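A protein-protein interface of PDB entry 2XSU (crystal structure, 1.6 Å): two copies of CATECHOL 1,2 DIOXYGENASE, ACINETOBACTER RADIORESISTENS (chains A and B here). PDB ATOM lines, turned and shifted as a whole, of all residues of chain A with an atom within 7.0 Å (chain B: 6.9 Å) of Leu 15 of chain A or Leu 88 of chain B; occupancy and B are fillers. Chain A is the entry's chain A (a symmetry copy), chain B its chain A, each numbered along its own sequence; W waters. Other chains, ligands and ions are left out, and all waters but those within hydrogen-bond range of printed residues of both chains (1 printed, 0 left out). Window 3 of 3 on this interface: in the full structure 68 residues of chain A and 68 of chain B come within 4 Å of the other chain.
The backbone NH (N) of His 6 of chain A sits at hydrogen-bond distance from the side-chain carboxylate (OE1) of Glu 48 of chain A.
A ring nitrogen (ND1) of His 84 of chain B is in hydrogen-bond range of the backbone carbonyl oxygen (O) of Phe 256 of chain B, at 3.2 Å.
O of Val 16 of chain A sits close to ND2 of Asn 20 of chain A, 3.5 Å away.
Among the printed residues, pairs that only touch across the chains: Met 19 of chain A with Phe 256 of chain B (3.2 Å), Ile 12 of chain A with Tyr 85 of chain B (3.4 Å), His 6 of chain A with Arg 89 of chain B (3.4 Å), His 6 of chain A with Glu 92 of chain B (3.4 Å), His 7 of chain A with Tyr 85 of chain B (3.4 Å), Met 19 of chain A with Gly 81 of chain B (3.7 Å), Phe 44 of chain A with Tyr 85 of chain B (3.7 Å), His 6 of chain A with Ala 93 of chain B (3.8 Å), Leu 15 of chain A with Leu 88 of chain B (3.9 Å), Phe 44 of chain A with Gly 81 of chain B (3.9 Å), Met 19 of chain A with Leu 80 of chain B (3.96 Å), Leu 15 of chain A with Tyr 85 of chain B (3.96 Å) and His 7 of chain A with Leu 88 of chain B (3.98 Å).
Of the printed residues of chain B, Asn 20 of chain A touches Leu 80.
Printed residues of chain B within 4 Å of Phe 44 of chain A: Gly 81 and Tyr 85.
Of the printed residues of chain B, Glu 48 of chain A touches Tyr 85 and Arg 89.
Leu 88 of chain B touches two residues of chain A.
The nearest residue of chain B that does not touch Leu 15 of chain A is His 84 of chain B (5.6 Å).
The nearest printed residue of chain A that does not touch Arg 89 of chain B is His 7 of chain A (4.1 Å).
Water W1 lies within hydrogen-bond range of the side-chain carboxylate of Glu 92 of chain B and the backbone carbonyl oxygen of His 6 of chain A.
No position is printed for both chains.
OE2 of Glu 48 of chain A sits at hydrogen-bond distance from OH of Tyr 85 of chain B, at 2.6 Å.
The guanidinium group (NE) of Arg 89 of chain B lies within salt-bridge range of the side-chain carboxylate (OE2) of Glu 48 of chain A, at 3.0 Å.
The side-chain amide nitrogen (ND2) of Asn 20 of chain A lies within hydrogen-bond range of the backbone carbonyl oxygen (O) of Leu 80 of chain B (3.0 Å).
Of the 17 printed residues of chain A, 8 touch a printed residue of chain B.
Printed residues of chain A that touch a printed residue of chain B: His 6, His 7, Ile 12, Leu 15, Met 19, Asn 20, Phe 44 and Glu 48.
Hydrophobic or aromatic side chains of chain A that line the printed part of chain B: His 6, His 7, Ile 12, Leu 15, Met 19 and Phe 44.
Among the printed residues, 16 pairs touch across the chains.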
ATOM      1  N   HIS A   6     -26.145  -9.917 -31.915  1.00  0.00           N
ATOM      2  CA  HIS A   6     -26.206  -9.124 -30.694  1.00  0.00           C
ATOM      3  C   HIS A   6     -25.384  -7.847 -30.752  1.00  0.00           C
ATOM      4  O   HIS A   6     -25.611  -6.920 -29.970  1.00  0.00           O
ATOM      5  CB  HIS A   6     -25.758  -9.996 -29.523  1.00  0.00           C
ATOM      6  CG  HIS A   6     -26.535 -11.268 -29.399  1.00  0.00           C
ATOM      7  ND1 HIS A   6     -27.916 -11.305 -29.419  1.00  0.00           N
ATOM      8  CD2 HIS A   6     -26.130 -12.549 -29.252  1.00  0.00           C
ATOM      9  CE1 HIS A   6     -28.322 -12.556 -29.282  1.00  0.00           C
ATOM     10  NE2 HIS A   6     -27.255 -13.331 -29.181  1.00  0.00           N
ATOM     11  N   HIS A   7     -24.410  -7.799 -31.664  1.00  0.00           N
ATOM     12  CA  HIS A   7     -23.574  -6.622 -31.883  1.00  0.00           C
ATOM     13  C   HIS A   7     -23.334  -6.459 -33.381  1.00  0.00           C
ATOM     14  O   HIS A   7     -23.191  -7.461 -34.086  1.00  0.00           O
ATOM     15  CB  HIS A   7     -22.215  -6.758 -31.169  1.00  0.00           C
ATOM     16  CG  HIS A   7     -22.318  -7.136 -29.720  1.00  0.00           C
ATOM     17  ND1 HIS A   7     -22.357  -6.207 -28.702  1.00  0.00           N
ATOM     18  CD2 HIS A   7     -22.397  -8.349 -29.126  1.00  0.00           C
ATOM     19  CE1 HIS A   7     -22.449  -6.836 -27.539  1.00  0.00           C
ATOM     20  NE2 HIS A   7     -22.496  -8.133 -27.771  1.00  0.00           N
ATOM     21  N   ARG A   9     -20.818  -4.400 -36.470  1.00  0.00           N
ATOM     22  CA  ARG A   9     -19.358  -4.230 -36.550  1.00  0.00           C
ATOM     23  C   ARG A   9     -18.900  -2.950 -35.862  1.00  0.00           C
ATOM     24  O   ARG A   9     -17.815  -2.942 -35.297  1.00  0.00           O
ATOM     25  CB  ARG A   9     -18.746  -4.362 -37.982  1.00  0.00           C
ATOM     26  CG  ARG A   9     -17.173  -4.305 -38.046  1.00  0.00           C
ATOM     27  CD  ARG A   9     -16.483  -5.495 -37.296  1.00  0.00           C
ATOM     28  NE  ARG A   9     -15.021  -5.481 -37.342  1.00  0.00           N
ATOM     29  CZ  ARG A   9     -14.275  -6.377 -38.003  1.00  0.00           C
ATOM     30  NH1 ARG A   9     -14.864  -7.341 -38.679  1.00  0.00           N
ATOM     31  NH2 ARG A   9     -12.942  -6.314 -37.968  1.00  0.00           N
ATOM     32  N   GLN A  10     -19.719  -1.893 -35.882  1.00  0.00           N
ATOM     33  CA  GLN A  10     -19.373  -0.653 -35.178  1.00  0.00           C
ATOM     34  C   GLN A  10     -19.227  -0.912 -33.680  1.00  0.00           C
ATOM     35  O   GLN A  10     -18.252  -0.460 -33.063  1.00  0.00           O
ATOM     36  CB  GLN A  10     -20.411   0.451 -35.437  1.00  0.00           C
ATOM     37  CG  GLN A  10     -20.252   1.166 -36.778  1.00  0.00           C
ATOM     38  CD  GLN A  10     -20.989   2.516 -36.820  1.00  0.00           C
ATOM     39  OE1 GLN A  10     -21.772   2.843 -35.917  1.00  0.00           O
ATOM     40  NE2 GLN A  10     -20.735   3.303 -37.870  1.00  0.00           N
ATOM     41  N   GLN A  11     -20.180  -1.656 -33.123  1.00  0.00           N
ATOM     42  CA  GLN A  11     -20.206  -1.970 -31.689  1.00  0.00           C
ATOM     43  C   GLN A  11     -19.042  -2.903 -31.352  1.00  0.00           C
ATOM     44  O   GLN A  11     -18.398  -2.730 -30.310  1.00  0.00           O
ATOM     45  CB  GLN A  11     -21.520  -2.615 -31.282  1.00  0.00           C
ATOM     46  CG  GLN A  11     -22.741  -1.669 -31.383  1.00  0.00           C
ATOM     47  CD  GLN A  11     -24.080  -2.413 -31.400  1.00  0.00           C
ATOM     48  OE1 GLN A  11     -24.212  -3.488 -31.974  1.00  0.00           O
ATOM     49  NE2 GLN A  11     -25.101  -1.805 -30.785  1.00  0.00           N
ATOM     50  N   ILE A  12     -18.747  -3.842 -32.250  1.00  0.00           N
ATOM     51  CA  ILE A  12     -17.589  -4.728 -32.060  1.00  0.00           C
ATOM     52  C   ILE A  12     -16.299  -3.914 -32.035  1.00  0.00           C
ATOM     53  O   ILE A  12     -15.449  -4.088 -31.154  1.00  0.00           O
ATOM     54  CB  ILE A  12     -17.535  -5.835 -33.173  1.00  0.00           C
ATOM     55  CG1 ILE A  12     -18.605  -6.908 -32.899  1.00  0.00           C
ATOM     56  CG2 ILE A  12     -16.101  -6.452 -33.334  1.00  0.00           C
ATOM     57  CD1 ILE A  12     -18.948  -7.840 -34.117  1.00  0.00           C
ATOM     58  N   ASP A  13     -16.112  -3.055 -33.044  1.00  0.00           N
ATOM     59  CA  ASP A  13     -14.901  -2.251 -33.118  1.00  0.00           C
ATOM     60  C   ASP A  13     -14.701  -1.369 -31.895  1.00  0.00           C
ATOM     61  O   ASP A  13     -13.568  -1.242 -31.409  1.00  0.00           O
ATOM     62  CB  ASP A  13     -14.908  -1.412 -34.404  1.00  0.00           C
ATOM     63  CG  ASP A  13     -14.660  -2.253 -35.627  1.00  0.00           C
ATOM     64  OD1 ASP A  13     -14.240  -3.432 -35.478  1.00  0.00           O
ATOM     65  OD2 ASP A  13     -14.895  -1.750 -36.752  1.00  0.00           O
ATOM     66  N   ALA A  14     -15.793  -0.820 -31.371  1.00  0.00           N
ATOM     67  CA  ALA A  14     -15.727   0.020 -30.179  1.00  0.00           C
ATOM     68  C   ALA A  14     -15.295  -0.800 -28.965  1.00  0.00           C
ATOM     69  O   ALA A  14     -14.424  -0.363 -28.208  1.00  0.00           O
ATOM     70  CB  ALA A  14     -17.074   0.714 -29.930  1.00  0.00           C
ATOM     71  N   LEU A  15     -15.869  -2.000 -28.813  1.00  0.00           N
ATOM     72  CA  LEU A  15     -15.474  -2.911 -27.715  1.00  0.00           C
ATOM     73  C   LEU A  15     -14.003  -3.347 -27.786  1.00  0.00           C
ATOM     74  O   LEU A  15     -13.277  -3.317 -26.787  1.00  0.00           O
ATOM     75  CB  LEU A  15     -16.379  -4.142 -27.713  1.00  0.00           C
ATOM     76  CG  LEU A  15     -17.794  -3.958 -27.181  1.00  0.00           C
ATOM     77  CD1 LEU A  15     -18.606  -5.211 -27.510  1.00  0.00           C
ATOM     78  CD2 LEU A  15     -17.764  -3.719 -25.674  1.00  0.00           C
ATOM     79  N   VAL A  16     -13.569  -3.745 -28.983  1.00  0.00           N
ATOM     80  CA  VAL A  16     -12.164  -4.148 -29.167  1.00  0.00           C
ATOM     81  C   VAL A  16     -11.210  -2.994 -28.818  1.00  0.00           C
ATOM     82  O   VAL A  16     -10.176  -3.222 -28.158  1.00  0.00           O
ATOM     83  CB  VAL A  16     -11.919  -4.683 -30.599  1.00  0.00           C
ATOM     84  CG1 VAL A  16     -10.418  -4.914 -30.843  1.00  0.00           C
ATOM     85  CG2 VAL A  16     -12.617  -6.006 -30.785  1.00  0.00           C
ATOM     86  N   LYS A  17     -11.573  -1.775 -29.244  1.00  0.00           N
ATOM     87  CA  LYS A  17     -10.768  -0.582 -28.944  1.00  0.00           C
ATOM     88  C   LYS A  17     -10.722  -0.317 -27.439  1.00  0.00           C
ATOM     89  O   LYS A  17      -9.648  -0.059 -26.875  1.00  0.00           O
ATOM     90  CB  LYS A  17     -11.301   0.637 -29.709  1.00  0.00           C
ATOM     91  CG  LYS A  17     -10.504   1.902 -29.462  1.00  0.00           C
ATOM     92  CD  LYS A  17     -11.040   3.048 -30.307  1.00  0.00           C
ATOM     93  CE  LYS A  17     -10.219   4.304 -30.070  1.00  0.00           C
ATOM     94  NZ  LYS A  17     -10.640   4.970 -28.808  1.00  0.00           N
ATOM     95  N   GLN A  18     -11.880  -0.380 -26.792  1.00  0.00           N
ATOM     96  CA  GLN A  18     -11.960  -0.126 -25.350  1.00  0.00           C
ATOM     97  C   GLN A  18     -11.069  -1.075 -24.563  1.00  0.00           C
ATOM     98  O   GLN A  18     -10.391  -0.664 -23.614  1.00  0.00           O
ATOM     99  CB  GLN A  18     -13.392  -0.290 -24.881  1.00  0.00           C
ATOM    100  CG  GLN A  18     -14.266   0.868 -25.288  1.00  0.00           C
ATOM    101  CD  GLN A  18     -15.740   0.556 -25.146  1.00  0.00           C
ATOM    102  OE1 GLN A  18     -16.135  -0.331 -24.380  1.00  0.00           O
ATOM    103  NE2 GLN A  18     -16.570   1.297 -25.885  1.00  0.00           N
ATOM    104  N   MET A  19     -11.062  -2.348 -24.973  1.00  0.00           N
ATOM    105  CA  MET A  19     -10.319  -3.376 -24.250  1.00  0.00           C
ATOM    106  C   MET A  19      -8.826  -3.434 -24.575  1.00  0.00           C
ATOM    107  O   MET A  19      -7.992  -3.706 -23.686  1.00  0.00           O
ATOM    108  CB  MET A  19     -10.996  -4.748 -24.443  1.00  0.00           C
ATOM    109  CG  MET A  19     -12.436  -4.791 -23.904  1.00  0.00           C
ATOM    110  SD  MET A  19     -13.226  -6.420 -23.944  1.00  0.00           S
ATOM    111  CE  MET A  19     -13.245  -6.711 -25.720  1.00  0.00           C
ATOM    112  N   ASN A  20      -8.463  -3.147 -25.825  1.00  0.00           N
ATOM    113  CA  ASN A  20      -7.107  -3.449 -26.294  1.00  0.00           C
ATOM    114  C   ASN A  20      -6.249  -2.245 -26.680  1.00  0.00           C
ATOM    115  O   ASN A  20      -5.020  -2.374 -26.839  1.00  0.00           O
ATOM    116  CB  ASN A  20      -7.141  -4.481 -27.439  1.00  0.00           C
ATOM    117  CG  ASN A  20      -7.535  -5.859 -26.936  1.00  0.00           C
ATOM    118  OD1 ASN A  20      -6.745  -6.536 -26.289  1.00  0.00           O
ATOM    119  ND2 ASN A  20      -8.788  -6.257 -27.196  1.00  0.00           N
ATOM    120  N   VAL A  21      -6.898  -1.085 -26.794  1.00  0.00           N
ATOM    121  CA  VAL A  21      -6.228   0.142 -27.263  1.00  0.00           C
ATOM    122  C   VAL A  21      -6.296   1.241 -26.191  1.00  0.00           C
ATOM    123  O   VAL A  21      -5.237   1.774 -25.796  1.00  0.00           O
ATOM    124  CB  VAL A  21      -6.840   0.638 -28.583  1.00  0.00           C
ATOM    125  CG1 VAL A  21      -6.223   1.969 -29.010  1.00  0.00           C
ATOM    126  CG2 VAL A  21      -6.654  -0.399 -29.687  1.00  0.00           C
ATOM    127  N   PHE A  44     -14.699 -11.675 -33.541  1.00  0.00           N
ATOM    128  CA  PHE A  44     -15.966 -11.310 -32.902  1.00  0.00           C
ATOM    129  C   PHE A  44     -17.111 -11.268 -33.922  1.00  0.00           C
ATOM    130  O   PHE A  44     -18.210 -11.728 -33.640  1.00  0.00           O
ATOM    131  CB  PHE A  44     -15.860  -9.944 -32.203  1.00  0.00           C
ATOM    132  CG  PHE A  44     -15.096  -9.938 -30.899  1.00  0.00           C
ATOM    133  CD1 PHE A  44     -14.318 -11.023 -30.465  1.00  0.00           C
ATOM    134  CD2 PHE A  44     -15.123  -8.788 -30.106  1.00  0.00           C
ATOM    135  CE1 PHE A  44     -13.586 -10.952 -29.257  1.00  0.00           C
ATOM    136  CE2 PHE A  44     -14.399  -8.723 -28.876  1.00  0.00           C
ATOM    137  CZ  PHE A  44     -13.632  -9.803 -28.471  1.00  0.00           C
ATOM    138  N   GLU A  48     -20.573 -13.547 -34.130  1.00  0.00           N
ATOM    139  CA  GLU A  48     -21.933 -13.024 -34.335  1.00  0.00           C
ATOM    140  C   GLU A  48     -22.604 -13.666 -35.554  1.00  0.00           C
ATOM    141  O   GLU A  48     -23.734 -14.171 -35.466  1.00  0.00           O
ATOM    142  CB  GLU A  48     -21.936 -11.514 -34.509  1.00  0.00           C
ATOM    143  CG  GLU A  48     -21.472 -10.743 -33.297  1.00  0.00           C
ATOM    144  CD  GLU A  48     -22.456 -10.820 -32.126  1.00  0.00           C
ATOM    145  OE1 GLU A  48     -23.641 -11.187 -32.317  1.00  0.00           O
ATOM    146  OE2 GLU A  48     -22.020 -10.497 -31.003  1.00  0.00           O
ATOM    147  N   LEU B  80      -7.547 -10.597 -23.882  1.00  0.00           N
ATOM    148  CA  LEU B  80      -7.921  -9.900 -25.113  1.00  0.00           C
ATOM    149  C   LEU B  80      -9.387  -9.474 -25.068  1.00  0.00           C
ATOM    150  O   LEU B  80      -9.837  -8.710 -25.919  1.00  0.00           O
ATOM    151  CB  LEU B  80      -7.643 -10.776 -26.346  1.00  0.00           C
ATOM    152  CG  LEU B  80      -6.154 -11.123 -26.540  1.00  0.00           C
ATOM    153  CD1 LEU B  80      -6.025 -11.941 -27.814  1.00  0.00           C
ATOM    154  CD2 LEU B  80      -5.233  -9.903 -26.599  1.00  0.00           C
ATOM    155  N   GLY B  81     -10.119  -9.993 -24.087  1.00  0.00           N
ATOM    156  CA  GLY B  81     -11.535  -9.659 -23.928  1.00  0.00           C
ATOM    157  C   GLY B  81     -12.514 -10.587 -24.640  1.00  0.00           C
ATOM    158  O   GLY B  81     -13.732 -10.363 -24.592  1.00  0.00           O
ATOM    159  N   GLU B  83     -13.231 -13.656 -23.639  1.00  0.00           N
ATOM    160  CA  GLU B  83     -14.029 -14.343 -22.631  1.00  0.00           C
ATOM    161  C   GLU B  83     -15.187 -13.440 -22.148  1.00  0.00           C
ATOM    162  O   GLU B  83     -16.341 -13.874 -22.089  1.00  0.00           O
ATOM    163  CB  GLU B  83     -13.113 -14.777 -21.459  1.00  0.00           C
ATOM    164  CG  GLU B  83     -13.831 -15.728 -20.517  1.00  0.00           C
ATOM    165  CD  GLU B  83     -12.880 -16.358 -19.470  1.00  0.00           C
ATOM    166  OE1 GLU B  83     -11.712 -15.907 -19.379  1.00  0.00           O
ATOM    167  OE2 GLU B  83     -13.328 -17.305 -18.774  1.00  0.00           O
ATOM    168  N   HIS B  84     -14.876 -12.177 -21.894  1.00  0.00           N
ATOM    169  CA  HIS B  84     -15.932 -11.217 -21.539  1.00  0.00           C
ATOM    170  C   HIS B  84     -16.969 -11.056 -22.671  1.00  0.00           C
ATOM    171  O   HIS B  84     -18.165 -10.950 -22.395  1.00  0.00           O
ATOM    172  CB  HIS B  84     -15.281  -9.866 -21.174  1.00  0.00           C
ATOM    173  CG  HIS B  84     -16.246  -8.749 -20.992  1.00  0.00           C
ATOM    174  ND1 HIS B  84     -17.251  -8.771 -20.042  1.00  0.00           N
ATOM    175  CD2 HIS B  84     -16.339  -7.555 -21.620  1.00  0.00           C
ATOM    176  CE1 HIS B  84     -17.937  -7.641 -20.116  1.00  0.00           C
ATOM    177  NE2 HIS B  84     -17.393  -6.876 -21.049  1.00  0.00           N
ATOM    178  N   TYR B  85     -16.513 -10.993 -23.924  1.00  0.00           N
ATOM    179  CA  TYR B  85     -17.414 -10.856 -25.083  1.00  0.00           C
ATOM    180  C   TYR B  85     -18.448 -11.983 -25.089  1.00  0.00           C
ATOM    181  O   TYR B  85     -19.622 -11.752 -25.409  1.00  0.00           O
ATOM    182  CB  TYR B  85     -16.592 -10.862 -26.381  1.00  0.00           C
ATOM    183  CG  TYR B  85     -17.413 -10.521 -27.623  1.00  0.00           C
ATOM    184  CD1 TYR B  85     -17.985  -9.259 -27.755  1.00  0.00           C
ATOM    185  CD2 TYR B  85     -17.594 -11.463 -28.640  1.00  0.00           C
ATOM    186  CE1 TYR B  85     -18.747  -8.929 -28.879  1.00  0.00           C
ATOM    187  CE2 TYR B  85     -18.377 -11.138 -29.775  1.00  0.00           C
ATOM    188  CZ  TYR B  85     -18.917  -9.855 -29.862  1.00  0.00           C
ATOM    189  OH  TYR B  85     -19.687  -9.449 -30.951  1.00  0.00           O
ATOM    190  N   LEU B  86     -18.035 -13.198 -24.741  1.00  0.00           N
ATOM    191  CA  LEU B  86     -18.968 -14.321 -24.736  1.00  0.00           C
ATOM    192  C   LEU B  86     -20.081 -14.062 -23.730  1.00  0.00           C
ATOM    193  O   LEU B  86     -21.239 -14.380 -24.007  1.00  0.00           O
ATOM    194  CB  LEU B  86     -18.260 -15.642 -24.430  1.00  0.00           C
ATOM    195  CG  LEU B  86     -17.135 -16.093 -25.353  1.00  0.00           C
ATOM    196  CD1 LEU B  86     -16.549 -17.418 -24.852  1.00  0.00           C
ATOM    197  CD2 LEU B  86     -17.674 -16.224 -26.768  1.00  0.00           C
ATOM    198  N   ASP B  87     -19.740 -13.479 -22.572  1.00  0.00           N
ATOM    199  CA  ASP B  87     -20.760 -13.083 -21.584  1.00  0.00           C
ATOM    200  C   ASP B  87     -21.660 -11.955 -22.101  1.00  0.00           C
ATOM    201  O   ASP B  87     -22.890 -11.968 -21.835  1.00  0.00           O
ATOM    202  CB  ASP B  87     -20.123 -12.631 -20.268  1.00  0.00           C
ATOM    203  CG  ASP B  87     -19.506 -13.763 -19.478  1.00  0.00           C
ATOM    204  OD1 ASP B  87     -19.739 -14.974 -19.772  1.00  0.00           O
ATOM    205  OD2 ASP B  87     -18.690 -13.414 -18.585  1.00  0.00           O
ATOM    206  N   LEU B  88     -21.081 -10.963 -22.787  1.00  0.00           N
ATOM    207  CA  LEU B  88     -21.907  -9.889 -23.389  1.00  0.00           C
ATOM    208  C   LEU B  88     -22.961 -10.506 -24.321  1.00  0.00           C
ATOM    209  O   LEU B  88     -24.145 -10.124 -24.274  1.00  0.00           O
ATOM    210  CB  LEU B  88     -21.059  -8.856 -24.135  1.00  0.00           C
ATOM    211  CG  LEU B  88     -20.128  -7.984 -23.286  1.00  0.00           C
ATOM    212  CD1 LEU B  88     -19.355  -7.042 -24.187  1.00  0.00           C
ATOM    213  CD2 LEU B  88     -20.882  -7.197 -22.213  1.00  0.00           C
ATOM    214  N   ARG B  89     -22.543 -11.468 -25.141  1.00  0.00           N
ATOM    215  CA  ARG B  89     -23.478 -12.183 -26.021  1.00  0.00           C
ATOM    216  C   ARG B  89     -24.532 -12.970 -25.241  1.00  0.00           C
ATOM    217  O   ARG B  89     -25.714 -12.937 -25.600  1.00  0.00           O
ATOM    218  CB  ARG B  89     -22.727 -13.089 -26.995  1.00  0.00           C
ATOM    219  CG  ARG B  89     -22.014 -12.294 -28.053  1.00  0.00           C
ATOM    220  CD  ARG B  89     -21.574 -13.203 -29.218  1.00  0.00           C
ATOM    221  NE  ARG B  89     -22.684 -13.284 -30.223  1.00  0.00           N
ATOM    222  CZ  ARG B  89     -23.294 -14.398 -30.618  1.00  0.00           C
ATOM    223  NH1 ARG B  89     -22.971 -15.606 -30.165  1.00  0.00           N
ATOM    224  NH2 ARG B  89     -24.276 -14.310 -31.496  1.00  0.00           N
ATOM    225  N   ALA B  90     -24.133 -13.647 -24.167  1.00  0.00           N
ATOM    226  CA  ALA B  90     -25.064 -14.449 -23.416  1.00  0.00           C
ATOM    227  C   ALA B  90     -26.102 -13.543 -22.755  1.00  0.00           C
ATOM    228  O   ALA B  90     -27.288 -13.896 -22.694  1.00  0.00           O
ATOM    229  CB  ALA B  90     -24.329 -15.289 -22.383  1.00  0.00           C
ATOM    230  N   ASP B  91     -25.648 -12.385 -22.262  1.00  0.00           N
ATOM    231  CA  ASP B  91     -26.562 -11.417 -21.628  1.00  0.00           C
ATOM    232  C   ASP B  91     -27.591 -10.907 -22.648  1.00  0.00           C
ATOM    233  O   ASP B  91     -28.773 -10.757 -22.301  1.00  0.00           O
ATOM    234  CB  ASP B  91     -25.810 -10.215 -21.021  1.00  0.00           C
ATOM    235  CG  ASP B  91     -25.182 -10.523 -19.662  1.00  0.00           C
ATOM    236  OD1 ASP B  91     -25.480 -11.556 -19.050  1.00  0.00           O
ATOM    237  OD2 ASP B  91     -24.386  -9.677 -19.208  1.00  0.00           O
ATOM    238  N   GLU B  92     -27.147 -10.654 -23.879  1.00  0.00           N
ATOM    239  CA  GLU B  92     -28.070 -10.157 -24.913  1.00  0.00           C
ATOM    240  C   GLU B  92     -29.051 -11.229 -25.365  1.00  0.00           C
ATOM    241  O   GLU B  92     -30.251 -10.916 -25.585  1.00  0.00           O
ATOM    242  CB  GLU B  92     -27.304  -9.561 -26.100  1.00  0.00           C
ATOM    243  CG  GLU B  92     -28.197  -8.794 -27.079  1.00  0.00           C
ATOM    244  CD  GLU B  92     -28.599  -7.378 -26.626  1.00  0.00           C
ATOM    245  OE1 GLU B  92     -28.288  -6.948 -25.494  1.00  0.00           O
ATOM    246  OE2 GLU B  92     -29.251  -6.677 -27.434  1.00  0.00           O
ATOM    247  N   ALA B  93     -28.578 -12.477 -25.501  1.00  0.00           N
ATOM    248  CA  ALA B  93     -29.484 -13.612 -25.759  1.00  0.00           C
ATOM    249  C   ALA B  93     -30.541 -13.758 -24.659  1.00  0.00           C
ATOM    250  O   ALA B  93     -31.729 -14.005 -24.958  1.00  0.00           O
ATOM    251  CB  ALA B  93     -28.702 -14.918 -25.920  1.00  0.00           C
ATOM    252  N   ARG B 105     -23.984 -12.662 -14.327  1.00  0.00           N
ATOM    253  CA  ARG B 105     -22.856 -13.518 -14.686  1.00  0.00           C
ATOM    254  C   ARG B 105     -21.577 -12.737 -14.934  1.00  0.00           C
ATOM    255  O   ARG B 105     -21.621 -11.563 -15.307  1.00  0.00           O
ATOM    256  CB  ARG B 105     -23.195 -14.341 -15.937  1.00  0.00           C
ATOM    257  CG  ARG B 105     -23.417 -13.473 -17.188  1.00  0.00           C
ATOM    258  CD  ARG B 105     -23.344 -14.243 -18.516  1.00  0.00           C
ATOM    259  NE  ARG B 105     -24.225 -15.398 -18.605  1.00  0.00           N
ATOM    260  CZ  ARG B 105     -25.502 -15.405 -19.000  1.00  0.00           C
ATOM    261  NH1 ARG B 105     -26.172 -14.296 -19.308  1.00  0.00           N
ATOM    262  NH2 ARG B 105     -26.135 -16.576 -19.053  1.00  0.00           N
ATOM    263  N   PHE B 256     -11.549  -7.686 -17.797  1.00  0.00           N
ATOM    264  CA  PHE B 256     -12.860  -7.001 -17.966  1.00  0.00           C
ATOM    265  C   PHE B 256     -14.067  -7.661 -17.295  1.00  0.00           C
ATOM    266  O   PHE B 256     -15.188  -7.601 -17.833  1.00  0.00           O
ATOM    267  CB  PHE B 256     -13.119  -6.759 -19.486  1.00  0.00           C
ATOM    268  CG  PHE B 256     -11.921  -6.240 -20.176  1.00  0.00           C
ATOM    269  CD1 PHE B 256     -11.577  -4.893 -20.047  1.00  0.00           C
ATOM    270  CD2 PHE B 256     -11.076  -7.104 -20.890  1.00  0.00           C
ATOM    271  CE1 PHE B 256     -10.412  -4.382 -20.650  1.00  0.00           C
ATOM    272  CE2 PHE B 256      -9.895  -6.604 -21.498  1.00  0.00           C
ATOM    273  CZ  PHE B 256      -9.577  -5.240 -21.348  1.00  0.00           C
ATOM    274  N   ARG B 259     -18.382  -5.994 -12.660  1.00  0.00           N
ATOM    275  CA  ARG B 259     -19.743  -5.523 -12.988  1.00  0.00           C
ATOM    276  C   ARG B 259     -20.414  -4.921 -11.801  1.00  0.00           C
ATOM    277  O   ARG B 259     -20.222  -5.379 -10.676  1.00  0.00           O
ATOM    278  CB  ARG B 259     -20.681  -6.714 -13.311  1.00  0.00           C
ATOM    279  CG  ARG B 259     -20.331  -7.500 -14.494  1.00  0.00           C
ATOM    280  CD  ARG B 259     -21.470  -8.437 -14.753  1.00  0.00           C
ATOM    281  NE  ARG B 259     -22.597  -7.759 -15.379  1.00  0.00           N
ATOM    282  CZ  ARG B 259     -23.350  -8.328 -16.308  1.00  0.00           C
ATOM    283  NH1 ARG B 259     -23.097  -9.581 -16.687  1.00  0.00           N
ATOM    284  NH2 ARG B 259     -24.347  -7.636 -16.878  1.00  0.00           N
HETATM  285  O   HOH W   1     -28.709  -6.701 -30.086  1.00  0.00           O
